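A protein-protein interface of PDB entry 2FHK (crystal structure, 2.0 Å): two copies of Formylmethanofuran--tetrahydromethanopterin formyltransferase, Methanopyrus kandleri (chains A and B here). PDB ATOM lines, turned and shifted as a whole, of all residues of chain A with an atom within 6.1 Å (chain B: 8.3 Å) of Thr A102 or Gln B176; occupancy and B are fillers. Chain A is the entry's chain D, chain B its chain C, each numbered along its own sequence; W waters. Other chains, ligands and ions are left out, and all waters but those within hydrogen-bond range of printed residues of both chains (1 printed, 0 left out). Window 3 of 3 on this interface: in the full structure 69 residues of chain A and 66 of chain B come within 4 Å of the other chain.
The side-chain hydroxyl of Tyr B244 sits at hydrogen-bond distance from the side-chain carboxylate of Glu A149.
N of Glu A149 sits at hydrogen-bond distance from O of Ala B206 (3.1 Å).
The backbone NH (N) of Glu A149 is in hydrogen-bond range of the backbone carbonyl oxygen (O) of Val B243 (3.2 Å).
SG of Cys B242 lies within hydrogen-bond range of O of Glu A149, 3.5 Å away.
The backbone NH (N) of Thr A102 lies within hydrogen-bond range of the side-chain carboxylate (OE1) of Glu A149.
The backbone NH (N) of Ile B171 lies within hydrogen-bond range of the backbone carbonyl oxygen (O) of Tyr B244 (2.7 Å).
The backbone NH (N) of Trp A32 is in hydrogen-bond range of the side-chain hydroxyl (OG) of Ser A29 (3.4 Å).
The side-chain hydroxyl of Tyr B244 is in hydrogen-bond range of the side-chain amide nitrogen of Gln B176.
The guanidinium group (NH2) of Arg A70 sits at hydrogen-bond distance from the backbone carbonyl oxygen (O) of Thr A102 (2.7 Å).
O of Cys B242 is in hydrogen-bond range of N of Ala B173, 3.0 Å away.
Among the printed residues, pairs that only touch across the chains: Trp A32 with Leu B180 (3.6 Å), Trp A32 with Ile B204 (3.7 Å), Ala A100 with Ala B206 (3.7 Å), Pro A101 with Leu B180 (3.5 Å), Pro A101 with Ile B204 (3.7 Å), Pro A101 with Ala B206 (3.8 Å), Thr A102 with Gln B176 (3.3 Å) and Thr A102 with Leu B180 (3.7 Å).
Of the printed residues of chain B, Trp A32 touches Leu B180 and Ile B204.
Printed residues of chain B within 4 Å of Thr A102: Gln B176 and Leu B180.
No residue of chain B comes within 4 Å of Ala A103.
Of the printed residues of chain A, Gln B176 touches Thr A102 (3.3 Å).
Of the printed residues of chain A, Leu B180 touches Trp A32 (3.6 Å), Pro A101 (3.5 Å) and Thr A102 (3.7 Å).
The nearest printed residue of chain B that does not touch Thr A102 is Tyr B244 (4.01 Å).
The nearest printed residue of chain A that does not touch Gln B176 is Glu A149 (4.01 Å).
Printed residues of chain B that touch a printed residue of chain A: Gln B176, Leu B180, Ile B204, Ala B206, Cys B242, Val B243 and Tyr B244.
Hydrophobic or aromatic side chains of chain B that line the printed part of chain A: Leu B180, Ile B204, Ala B206 and Tyr B244.
Along chain B the printed residues that touch a printed residue of chain A span positions 176 to 244.
Of the 13 printed residues of chain A, 5 touch a printed residue of chain B.
Printed residues of chain A that touch a printed residue of chain B: Trp A32, Ala A100, Pro A101, Thr A102 and Glu A149.
Hydrophobic or aromatic side chains of chain A within 4 Å of the printed part of chain B: Trp A32 and Pro A101.
Among the printed residues, 12 pairs touch across the chains.
No position is printed for both chains.
Water W1 lies within hydrogen-bond range of the backbone carbonyl oxygen of Glu A149 (2.7 Å) and the backbone carbonyl oxygen of Lys B241 (2.8 Å).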
ATOM      1  N   THR A  26     -24.461  19.867  -7.826  1.00  0.00           N
ATOM      2  CA  THR A  26     -23.232  19.150  -7.499  1.00  0.00           C
ATOM      3  C   THR A  26     -22.442  19.977  -6.482  1.00  0.00           C
ATOM      4  O   THR A  26     -22.665  21.182  -6.347  1.00  0.00           O
ATOM      5  CB  THR A  26     -22.369  18.846  -8.745  1.00  0.00           C
ATOM      6  OG1 THR A  26     -21.818  20.059  -9.260  1.00  0.00           O
ATOM      7  CG2 THR A  26     -23.194  18.169  -9.840  1.00  0.00           C
ATOM      8  N   ALA A  27     -21.552  19.318  -5.746  1.00  0.00           N
ATOM      9  CA  ALA A  27     -20.753  19.973  -4.707  1.00  0.00           C
ATOM     10  C   ALA A  27     -19.531  19.112  -4.408  1.00  0.00           C
ATOM     11  O   ALA A  27     -19.388  18.033  -4.972  1.00  0.00           O
ATOM     12  CB  ALA A  27     -21.586  20.174  -3.450  1.00  0.00           C
ATOM     13  N   ALA A  28     -18.662  19.575  -3.515  1.00  0.00           N
ATOM     14  CA  ALA A  28     -17.425  18.848  -3.188  1.00  0.00           C
ATOM     15  C   ALA A  28     -17.684  17.469  -2.592  1.00  0.00           C
ATOM     16  O   ALA A  28     -16.865  16.562  -2.746  1.00  0.00           O
ATOM     17  CB  ALA A  28     -16.546  19.673  -2.251  1.00  0.00           C
ATOM     18  N   SER A  29     -18.816  17.327  -1.901  1.00  0.00           N
ATOM     19  CA  SER A  29     -19.252  16.045  -1.345  1.00  0.00           C
ATOM     20  C   SER A  29     -20.775  15.954  -1.349  1.00  0.00           C
ATOM     21  O   SER A  29     -21.458  16.944  -1.614  1.00  0.00           O
ATOM     22  CB  SER A  29     -18.709  15.845   0.078  1.00  0.00           C
ATOM     23  OG  SER A  29     -19.353  16.700   1.011  1.00  0.00           O
ATOM     24  N   TRP A  32     -22.213  18.484   1.326  1.00  0.00           N
ATOM     25  CA  TRP A  32     -22.371  19.880   0.923  1.00  0.00           C
ATOM     26  C   TRP A  32     -23.442  20.079  -0.145  1.00  0.00           C
ATOM     27  O   TRP A  32     -24.092  21.128  -0.192  1.00  0.00           O
ATOM     28  CB  TRP A  32     -21.016  20.463   0.491  1.00  0.00           C
ATOM     29  CG  TRP A  32     -20.095  20.671   1.664  1.00  0.00           C
ATOM     30  CD1 TRP A  32     -18.927  20.003   1.924  1.00  0.00           C
ATOM     31  CD2 TRP A  32     -20.284  21.586   2.751  1.00  0.00           C
ATOM     32  NE1 TRP A  32     -18.378  20.452   3.103  1.00  0.00           N
ATOM     33  CE2 TRP A  32     -19.189  21.425   3.629  1.00  0.00           C
ATOM     34  CE3 TRP A  32     -21.276  22.530   3.067  1.00  0.00           C
ATOM     35  CZ2 TRP A  32     -19.054  22.171   4.805  1.00  0.00           C
ATOM     36  CZ3 TRP A  32     -21.143  23.272   4.233  1.00  0.00           C
ATOM     37  CH2 TRP A  32     -20.034  23.087   5.090  1.00  0.00           C
ATOM     38  N   ALA A  33     -23.630  19.078  -1.000  1.00  0.00           N
ATOM     39  CA  ALA A  33     -24.736  19.087  -1.948  1.00  0.00           C
ATOM     40  C   ALA A  33     -26.056  19.088  -1.185  1.00  0.00           C
ATOM     41  O   ALA A  33     -26.928  19.907  -1.473  1.00  0.00           O
ATOM     42  CB  ALA A  33     -24.660  17.901  -2.920  1.00  0.00           C
ATOM     43  N   ARG A  70     -18.353  15.531  -9.948  1.00  0.00           N
ATOM     44  CA  ARG A  70     -18.517  15.681  -8.498  1.00  0.00           C
ATOM     45  C   ARG A  70     -19.846  15.077  -8.031  1.00  0.00           C
ATOM     46  O   ARG A  70     -20.777  14.968  -8.830  1.00  0.00           O
ATOM     47  CB  ARG A  70     -18.435  17.158  -8.095  1.00  0.00           C
ATOM     48  CG  ARG A  70     -17.106  17.845  -8.412  1.00  0.00           C
ATOM     49  CD  ARG A  70     -17.024  19.221  -7.761  1.00  0.00           C
ATOM     50  NE  ARG A  70     -18.216  20.011  -8.040  1.00  0.00           N
ATOM     51  CZ  ARG A  70     -18.573  21.105  -7.379  1.00  0.00           C
ATOM     52  NH1 ARG A  70     -19.686  21.735  -7.724  1.00  0.00           N
ATOM     53  NH2 ARG A  70     -17.824  21.574  -6.388  1.00  0.00           N
ATOM     54  N   ALA A 100     -24.199  28.633  -1.243  1.00  0.00           N
ATOM     55  CA  ALA A 100     -23.793  27.400  -0.559  1.00  0.00           C
ATOM     56  C   ALA A 100     -22.384  26.979  -0.958  1.00  0.00           C
ATOM     57  O   ALA A 100     -22.052  26.966  -2.145  1.00  0.00           O
ATOM     58  CB  ALA A 100     -24.771  26.285  -0.861  1.00  0.00           C
ATOM     59  N   PRO A 101     -21.547  26.617   0.026  1.00  0.00           N
ATOM     60  CA  PRO A 101     -20.175  26.209  -0.280  1.00  0.00           C
ATOM     61  C   PRO A 101     -20.056  25.118  -1.363  1.00  0.00           C
ATOM     62  O   PRO A 101     -20.715  24.069  -1.285  1.00  0.00           O
ATOM     63  CB  PRO A 101     -19.664  25.690   1.068  1.00  0.00           C
ATOM     64  CG  PRO A 101     -20.452  26.453   2.076  1.00  0.00           C
ATOM     65  CD  PRO A 101     -21.818  26.573   1.477  1.00  0.00           C
ATOM     66  N   THR A 102     -19.227  25.399  -2.372  1.00  0.00           N
ATOM     67  CA  THR A 102     -18.840  24.446  -3.435  1.00  0.00           C
ATOM     68  C   THR A 102     -19.925  24.008  -4.418  1.00  0.00           C
ATOM     69  O   THR A 102     -19.612  23.317  -5.387  1.00  0.00           O
ATOM     70  CB  THR A 102     -18.082  23.162  -2.895  1.00  0.00           C
ATOM     71  OG1 THR A 102     -19.001  22.264  -2.257  1.00  0.00           O
ATOM     72  CG2 THR A 102     -16.984  23.538  -1.918  1.00  0.00           C
ATOM     73  N   ALA A 103     -21.176  24.418  -4.194  1.00  0.00           N
ATOM     74  CA  ALA A 103     -22.304  23.909  -4.978  1.00  0.00           C
ATOM     75  C   ALA A 103     -22.412  24.541  -6.372  1.00  0.00           C
ATOM     76  O   ALA A 103     -22.235  25.754  -6.533  1.00  0.00           O
ATOM     77  CB  ALA A 103     -23.622  24.078  -4.202  1.00  0.00           C
ATOM     78  N   SER A 104     -22.694  23.704  -7.369  1.00  0.00           N
ATOM     79  CA  SER A 104     -22.978  24.154  -8.732  1.00  0.00           C
ATOM     80  C   SER A 104     -24.410  23.757  -9.091  1.00  0.00           C
ATOM     81  O   SER A 104     -24.981  22.860  -8.474  1.00  0.00           O
ATOM     82  CB  SER A 104     -21.993  23.524  -9.728  1.00  0.00           C
ATOM     83  OG  SER A 104     -20.645  23.767  -9.354  1.00  0.00           O
ATOM     84  N   GLU A 149     -15.506  32.675  -2.727  1.00  0.00           N
ATOM     85  CA  GLU A 149     -15.000  31.303  -2.613  1.00  0.00           C
ATOM     86  C   GLU A 149     -14.097  30.918  -3.793  1.00  0.00           C
ATOM     87  O   GLU A 149     -13.152  30.130  -3.642  1.00  0.00           O
ATOM     88  CB  GLU A 149     -16.165  30.307  -2.518  1.00  0.00           C
ATOM     89  CG  GLU A 149     -15.742  28.830  -2.538  1.00  0.00           C
ATOM     90  CD  GLU A 149     -16.905  27.877  -2.804  1.00  0.00           C
ATOM     91  OE1 GLU A 149     -17.302  27.162  -1.861  1.00  0.00           O
ATOM     92  OE2 GLU A 149     -17.421  27.844  -3.947  1.00  0.00           O
ATOM     93  N   ILE B 171     -13.236  34.586   6.429  1.00  0.00           N
ATOM     94  CA  ILE B 171     -12.127  33.649   6.606  1.00  0.00           C
ATOM     95  C   ILE B 171     -11.357  33.631   5.306  1.00  0.00           C
ATOM     96  O   ILE B 171     -11.890  33.224   4.280  1.00  0.00           O
ATOM     97  CB  ILE B 171     -12.624  32.235   6.927  1.00  0.00           C
ATOM     98  CG1 ILE B 171     -13.446  32.246   8.215  1.00  0.00           C
ATOM     99  CG2 ILE B 171     -11.442  31.250   7.023  1.00  0.00           C
ATOM    100  CD1 ILE B 171     -14.309  31.022   8.397  1.00  0.00           C
ATOM    101  N   ALA B 173      -8.282  32.033   3.430  1.00  0.00           N
ATOM    102  CA  ALA B 173      -7.437  30.849   3.515  1.00  0.00           C
ATOM    103  C   ALA B 173      -6.585  30.633   2.270  1.00  0.00           C
ATOM    104  O   ALA B 173      -6.809  31.270   1.223  1.00  0.00           O
ATOM    105  CB  ALA B 173      -8.292  29.625   3.798  1.00  0.00           C
ATOM    106  N   GLU B 174      -5.613  29.731   2.402  1.00  0.00           N
ATOM    107  CA  GLU B 174      -4.678  29.372   1.331  1.00  0.00           C
ATOM    108  C   GLU B 174      -5.328  28.589   0.176  1.00  0.00           C
ATOM    109  O   GLU B 174      -4.784  28.524  -0.932  1.00  0.00           O
ATOM    110  CB  GLU B 174      -3.498  28.574   1.913  1.00  0.00           C
ATOM    111  CG  GLU B 174      -3.891  27.183   2.436  1.00  0.00           C
ATOM    112  CD  GLU B 174      -2.707  26.350   2.907  1.00  0.00           C
ATOM    113  OE1 GLU B 174      -1.690  26.930   3.352  1.00  0.00           O
ATOM    114  OE2 GLU B 174      -2.804  25.104   2.841  1.00  0.00           O
ATOM    115  N   SER B 175      -6.486  27.989   0.445  1.00  0.00           N
ATOM    116  CA  SER B 175      -7.210  27.218  -0.554  1.00  0.00           C
ATOM    117  C   SER B 175      -8.689  27.119  -0.177  1.00  0.00           C
ATOM    118  O   SER B 175      -9.066  27.423   0.957  1.00  0.00           O
ATOM    119  CB  SER B 175      -6.604  25.816  -0.686  1.00  0.00           C
ATOM    120  OG  SER B 175      -6.804  25.056   0.495  1.00  0.00           O
ATOM    121  N   GLN B 176      -9.519  26.712  -1.133  1.00  0.00           N
ATOM    122  CA  GLN B 176     -10.933  26.438  -0.861  1.00  0.00           C
ATOM    123  C   GLN B 176     -11.130  25.343   0.208  1.00  0.00           C
ATOM    124  O   GLN B 176     -11.813  25.575   1.201  1.00  0.00           O
ATOM    125  CB  GLN B 176     -11.700  26.149  -2.159  1.00  0.00           C
ATOM    126  CG  GLN B 176     -13.174  25.804  -1.969  1.00  0.00           C
ATOM    127  CD  GLN B 176     -13.388  24.328  -1.728  1.00  0.00           C
ATOM    128  OE1 GLN B 176     -13.005  23.501  -2.545  1.00  0.00           O
ATOM    129  NE2 GLN B 176     -14.009  23.992  -0.606  1.00  0.00           N
ATOM    130  N   PRO B 177     -10.523  24.157   0.029  1.00  0.00           N
ATOM    131  CA  PRO B 177     -10.671  23.166   1.094  1.00  0.00           C
ATOM    132  C   PRO B 177     -10.290  23.668   2.497  1.00  0.00           C
ATOM    133  O   PRO B 177     -10.985  23.351   3.474  1.00  0.00           O
ATOM    134  CB  PRO B 177      -9.728  22.039   0.644  1.00  0.00           C
ATOM    135  CG  PRO B 177      -9.721  22.147  -0.824  1.00  0.00           C
ATOM    136  CD  PRO B 177      -9.702  23.629  -1.077  1.00  0.00           C
ATOM    137  N   ALA B 178      -9.209  24.439   2.602  1.00  0.00           N
ATOM    138  CA  ALA B 178      -8.761  24.959   3.897  1.00  0.00           C
ATOM    139  C   ALA B 178      -9.762  25.943   4.471  1.00  0.00           C
ATOM    140  O   ALA B 178     -10.042  25.923   5.671  1.00  0.00           O
ATOM    141  CB  ALA B 178      -7.373  25.598   3.798  1.00  0.00           C
ATOM    142  N   GLY B 179     -10.306  26.787   3.606  1.00  0.00           N
ATOM    143  CA  GLY B 179     -11.284  27.785   4.022  1.00  0.00           C
ATOM    144  C   GLY B 179     -12.558  27.150   4.544  1.00  0.00           C
ATOM    145  O   GLY B 179     -13.110  27.604   5.539  1.00  0.00           O
ATOM    146  N   LEU B 180     -13.019  26.103   3.859  1.00  0.00           N
ATOM    147  CA  LEU B 180     -14.265  25.435   4.200  1.00  0.00           C
ATOM    148  C   LEU B 180     -14.135  24.627   5.489  1.00  0.00           C
ATOM    149  O   LEU B 180     -15.063  24.595   6.298  1.00  0.00           O
ATOM    150  CB  LEU B 180     -14.753  24.563   3.033  1.00  0.00           C
ATOM    151  CG  LEU B 180     -16.159  23.952   3.096  1.00  0.00           C
ATOM    152  CD1 LEU B 180     -17.200  24.991   3.476  1.00  0.00           C
ATOM    153  CD2 LEU B 180     -16.529  23.259   1.776  1.00  0.00           C
ATOM    154  N   GLN B 181     -12.990  23.982   5.688  1.00  0.00           N
ATOM    155  CA  GLN B 181     -12.734  23.291   6.958  1.00  0.00           C
ATOM    156  C   GLN B 181     -12.773  24.286   8.116  1.00  0.00           C
ATOM    157  O   GLN B 181     -13.393  24.016   9.146  1.00  0.00           O
ATOM    158  CB  GLN B 181     -11.410  22.514   6.928  1.00  0.00           C
ATOM    159  CG  GLN B 181     -11.175  21.598   8.158  1.00  0.00           C
ATOM    160  CD  GLN B 181     -10.033  20.637   7.950  1.00  0.00           C
ATOM    161  OE1 GLN B 181     -10.074  19.797   7.052  1.00  0.00           O
ATOM    162  NE2 GLN B 181      -8.998  20.752   8.779  1.00  0.00           N
ATOM    163  N   ALA B 182     -12.134  25.446   7.940  1.00  0.00           N
ATOM    164  CA  ALA B 182     -12.120  26.463   8.997  1.00  0.00           C
ATOM    165  C   ALA B 182     -13.521  27.018   9.234  1.00  0.00           C
ATOM    166  O   ALA B 182     -13.921  27.215  10.371  1.00  0.00           O
ATOM    167  CB  ALA B 182     -11.160  27.592   8.655  1.00  0.00           C
ATOM    168  N   ALA B 183     -14.249  27.262   8.147  1.00  0.00           N
ATOM    169  CA  ALA B 183     -15.611  27.801   8.203  1.00  0.00           C
ATOM    170  C   ALA B 183     -16.599  26.869   8.913  1.00  0.00           C
ATOM    171  O   ALA B 183     -17.478  27.331   9.627  1.00  0.00           O
ATOM    172  CB  ALA B 183     -16.100  28.126   6.800  1.00  0.00           C
ATOM    173  N   ILE B 204     -22.609  29.226   6.138  1.00  0.00           N
ATOM    174  CA  ILE B 204     -21.489  29.787   5.372  1.00  0.00           C
ATOM    175  C   ILE B 204     -21.944  30.465   4.061  1.00  0.00           C
ATOM    176  O   ILE B 204     -22.777  29.918   3.331  1.00  0.00           O
ATOM    177  CB  ILE B 204     -20.445  28.672   5.064  1.00  0.00           C
ATOM    178  CG1 ILE B 204     -20.002  27.979   6.366  1.00  0.00           C
ATOM    179  CG2 ILE B 204     -19.235  29.245   4.330  1.00  0.00           C
ATOM    180  CD1 ILE B 204     -19.485  26.534   6.189  1.00  0.00           C
ATOM    181  N   VAL B 205     -21.398  31.657   3.785  1.00  0.00           N
ATOM    182  CA  VAL B 205     -21.621  32.363   2.514  1.00  0.00           C
ATOM    183  C   VAL B 205     -20.446  32.108   1.569  1.00  0.00           C
ATOM    184  O   VAL B 205     -19.313  32.501   1.858  1.00  0.00           O
ATOM    185  CB  VAL B 205     -21.746  33.909   2.693  1.00  0.00           C
ATOM    186  CG1 VAL B 205     -22.348  34.550   1.435  1.00  0.00           C
ATOM    187  CG2 VAL B 205     -22.569  34.262   3.915  1.00  0.00           C
ATOM    188  N   ALA B 206     -20.714  31.455   0.443  1.00  0.00           N
ATOM    189  CA  ALA B 206     -19.678  31.216  -0.556  1.00  0.00           C
ATOM    190  C   ALA B 206     -19.571  32.383  -1.540  1.00  0.00           C
ATOM    191  O   ALA B 206     -18.592  32.481  -2.286  1.00  0.00           O
ATOM    192  CB  ALA B 206     -19.935  29.903  -1.287  1.00  0.00           C
ATOM    193  N   SER B 207     -20.574  33.265  -1.520  1.00  0.00           N
ATOM    194  CA  SER B 207     -20.693  34.349  -2.494  1.00  0.00           C
ATOM    195  C   SER B 207     -21.113  35.667  -1.825  1.00  0.00           C
ATOM    196  O   SER B 207     -22.238  36.160  -2.020  1.00  0.00           O
ATOM    197  CB  SER B 207     -21.678  33.961  -3.600  1.00  0.00           C
ATOM    198  OG  SER B 207     -22.966  33.749  -3.061  1.00  0.00           O
ATOM    199  N   PRO B 229     -10.980  35.690  -5.607  1.00  0.00           N
ATOM    200  CA  PRO B 229      -9.623  35.289  -5.990  1.00  0.00           C
ATOM    201  C   PRO B 229      -9.393  35.144  -7.506  1.00  0.00           C
ATOM    202  O   PRO B 229      -8.244  35.208  -7.949  1.00  0.00           O
ATOM    203  CB  PRO B 229      -9.422  33.952  -5.262  1.00  0.00           C
ATOM    204  CG  PRO B 229     -10.786  33.441  -5.008  1.00  0.00           C
ATOM    205  CD  PRO B 229     -11.675  34.632  -4.849  1.00  0.00           C
ATOM    206  N   VAL B 240      -3.760  34.173  -0.401  1.00  0.00           N
ATOM    207  CA  VAL B 240      -5.186  33.920  -0.190  1.00  0.00           C
ATOM    208  C   VAL B 240      -5.841  33.489  -1.508  1.00  0.00           C
ATOM    209  O   VAL B 240      -5.954  34.285  -2.451  1.00  0.00           O
ATOM    210  CB  VAL B 240      -5.931  35.141   0.430  1.00  0.00           C
ATOM    211  CG1 VAL B 240      -7.447  34.906   0.449  1.00  0.00           C
ATOM    212  CG2 VAL B 240      -5.430  35.423   1.839  1.00  0.00           C
ATOM    213  N   LYS B 241      -6.260  32.225  -1.561  1.00  0.00           N
ATOM    214  CA  LYS B 241      -6.888  31.654  -2.758  1.00  0.00           C
ATOM    215  C   LYS B 241      -8.384  31.369  -2.574  1.00  0.00           C
ATOM    216  O   LYS B 241      -9.062  30.928  -3.515  1.00  0.00           O
ATOM    217  CB  LYS B 241      -6.158  30.383  -3.198  1.00  0.00           C
ATOM    218  CG  LYS B 241      -4.698  30.585  -3.591  1.00  0.00           C
ATOM    219  N   CYS B 242      -8.892  31.619  -1.367  1.00  0.00           N
ATOM    220  CA  CYS B 242     -10.320  31.457  -1.069  1.00  0.00           C
ATOM    221  C   CYS B 242     -10.772  32.323   0.103  1.00  0.00           C
ATOM    222  O   CYS B 242     -10.069  32.455   1.103  1.00  0.00           O
ATOM    223  CB  CYS B 242     -10.644  29.989  -0.775  1.00  0.00           C
ATOM    224  SG  CYS B 242     -12.375  29.655  -0.311  1.00  0.00           S
ATOM    225  N   VAL B 243     -11.965  32.892  -0.028  1.00  0.00           N
ATOM    226  CA  VAL B 243     -12.595  33.658   1.050  1.00  0.00           C
ATOM    227  C   VAL B 243     -13.995  33.097   1.330  1.00  0.00           C
ATOM    228  O   VAL B 243     -14.786  32.890   0.403  1.00  0.00           O
ATOM    229  CB  VAL B 243     -12.682  35.174   0.701  1.00  0.00           C
ATOM    230  CG1 VAL B 243     -13.511  35.943   1.741  1.00  0.00           C
ATOM    231  CG2 VAL B 243     -11.297  35.779   0.585  1.00  0.00           C
ATOM    232  N   TYR B 244     -14.285  32.829   2.599  1.00  0.00           N
ATOM    233  CA  TYR B 244     -15.658  32.556   3.036  1.00  0.00           C
ATOM    234  C   TYR B 244     -16.138  33.630   4.005  1.00  0.00           C
ATOM    235  O   TYR B 244     -15.345  34.211   4.747  1.00  0.00           O
ATOM    236  CB  TYR B 244     -15.770  31.184   3.705  1.00  0.00           C
ATOM    237  CG  TYR B 244     -15.774  30.015   2.751  1.00  0.00           C
ATOM    238  CD1 TYR B 244     -14.677  29.159   2.674  1.00  0.00           C
ATOM    239  CD2 TYR B 244     -16.876  29.753   1.931  1.00  0.00           C
ATOM    240  CE1 TYR B 244     -14.678  28.073   1.808  1.00  0.00           C
ATOM    241  CE2 TYR B 244     -16.886  28.659   1.060  1.00  0.00           C
ATOM    242  CZ  TYR B 244     -15.774  27.827   1.009  1.00  0.00           C
ATOM    243  OH  TYR B 244     -15.761  26.753   0.151  1.00  0.00           O
ATOM    244  N   PRO B 271      -5.995  24.400   9.913  1.00  0.00           N
ATOM    245  CA  PRO B 271      -4.819  24.738   9.094  1.00  0.00           C
ATOM    246  C   PRO B 271      -5.132  25.514   7.813  1.00  0.00           C
ATOM    247  O   PRO B 271      -6.206  25.352   7.227  1.00  0.00           O
ATOM    248  CB  PRO B 271      -4.242  23.364   8.728  1.00  0.00           C
ATOM    249  CG  PRO B 271      -5.414  22.436   8.804  1.00  0.00           C
ATOM    250  CD  PRO B 271      -6.255  22.945   9.921  1.00  0.00           C
ATOM    251  N   GLY B 272      -4.190  26.350   7.389  1.00  0.00           N
ATOM    252  CA  GLY B 272      -4.267  26.985   6.078  1.00  0.00           C
ATOM    253  C   GLY B 272      -5.039  28.288   6.046  1.00  0.00           C
ATOM    254  O   GLY B 272      -5.325  28.824   4.969  1.00  0.00           O
HETATM  255  O   HOH W   1     -10.890  29.257  -4.772  1.00  0.00           O
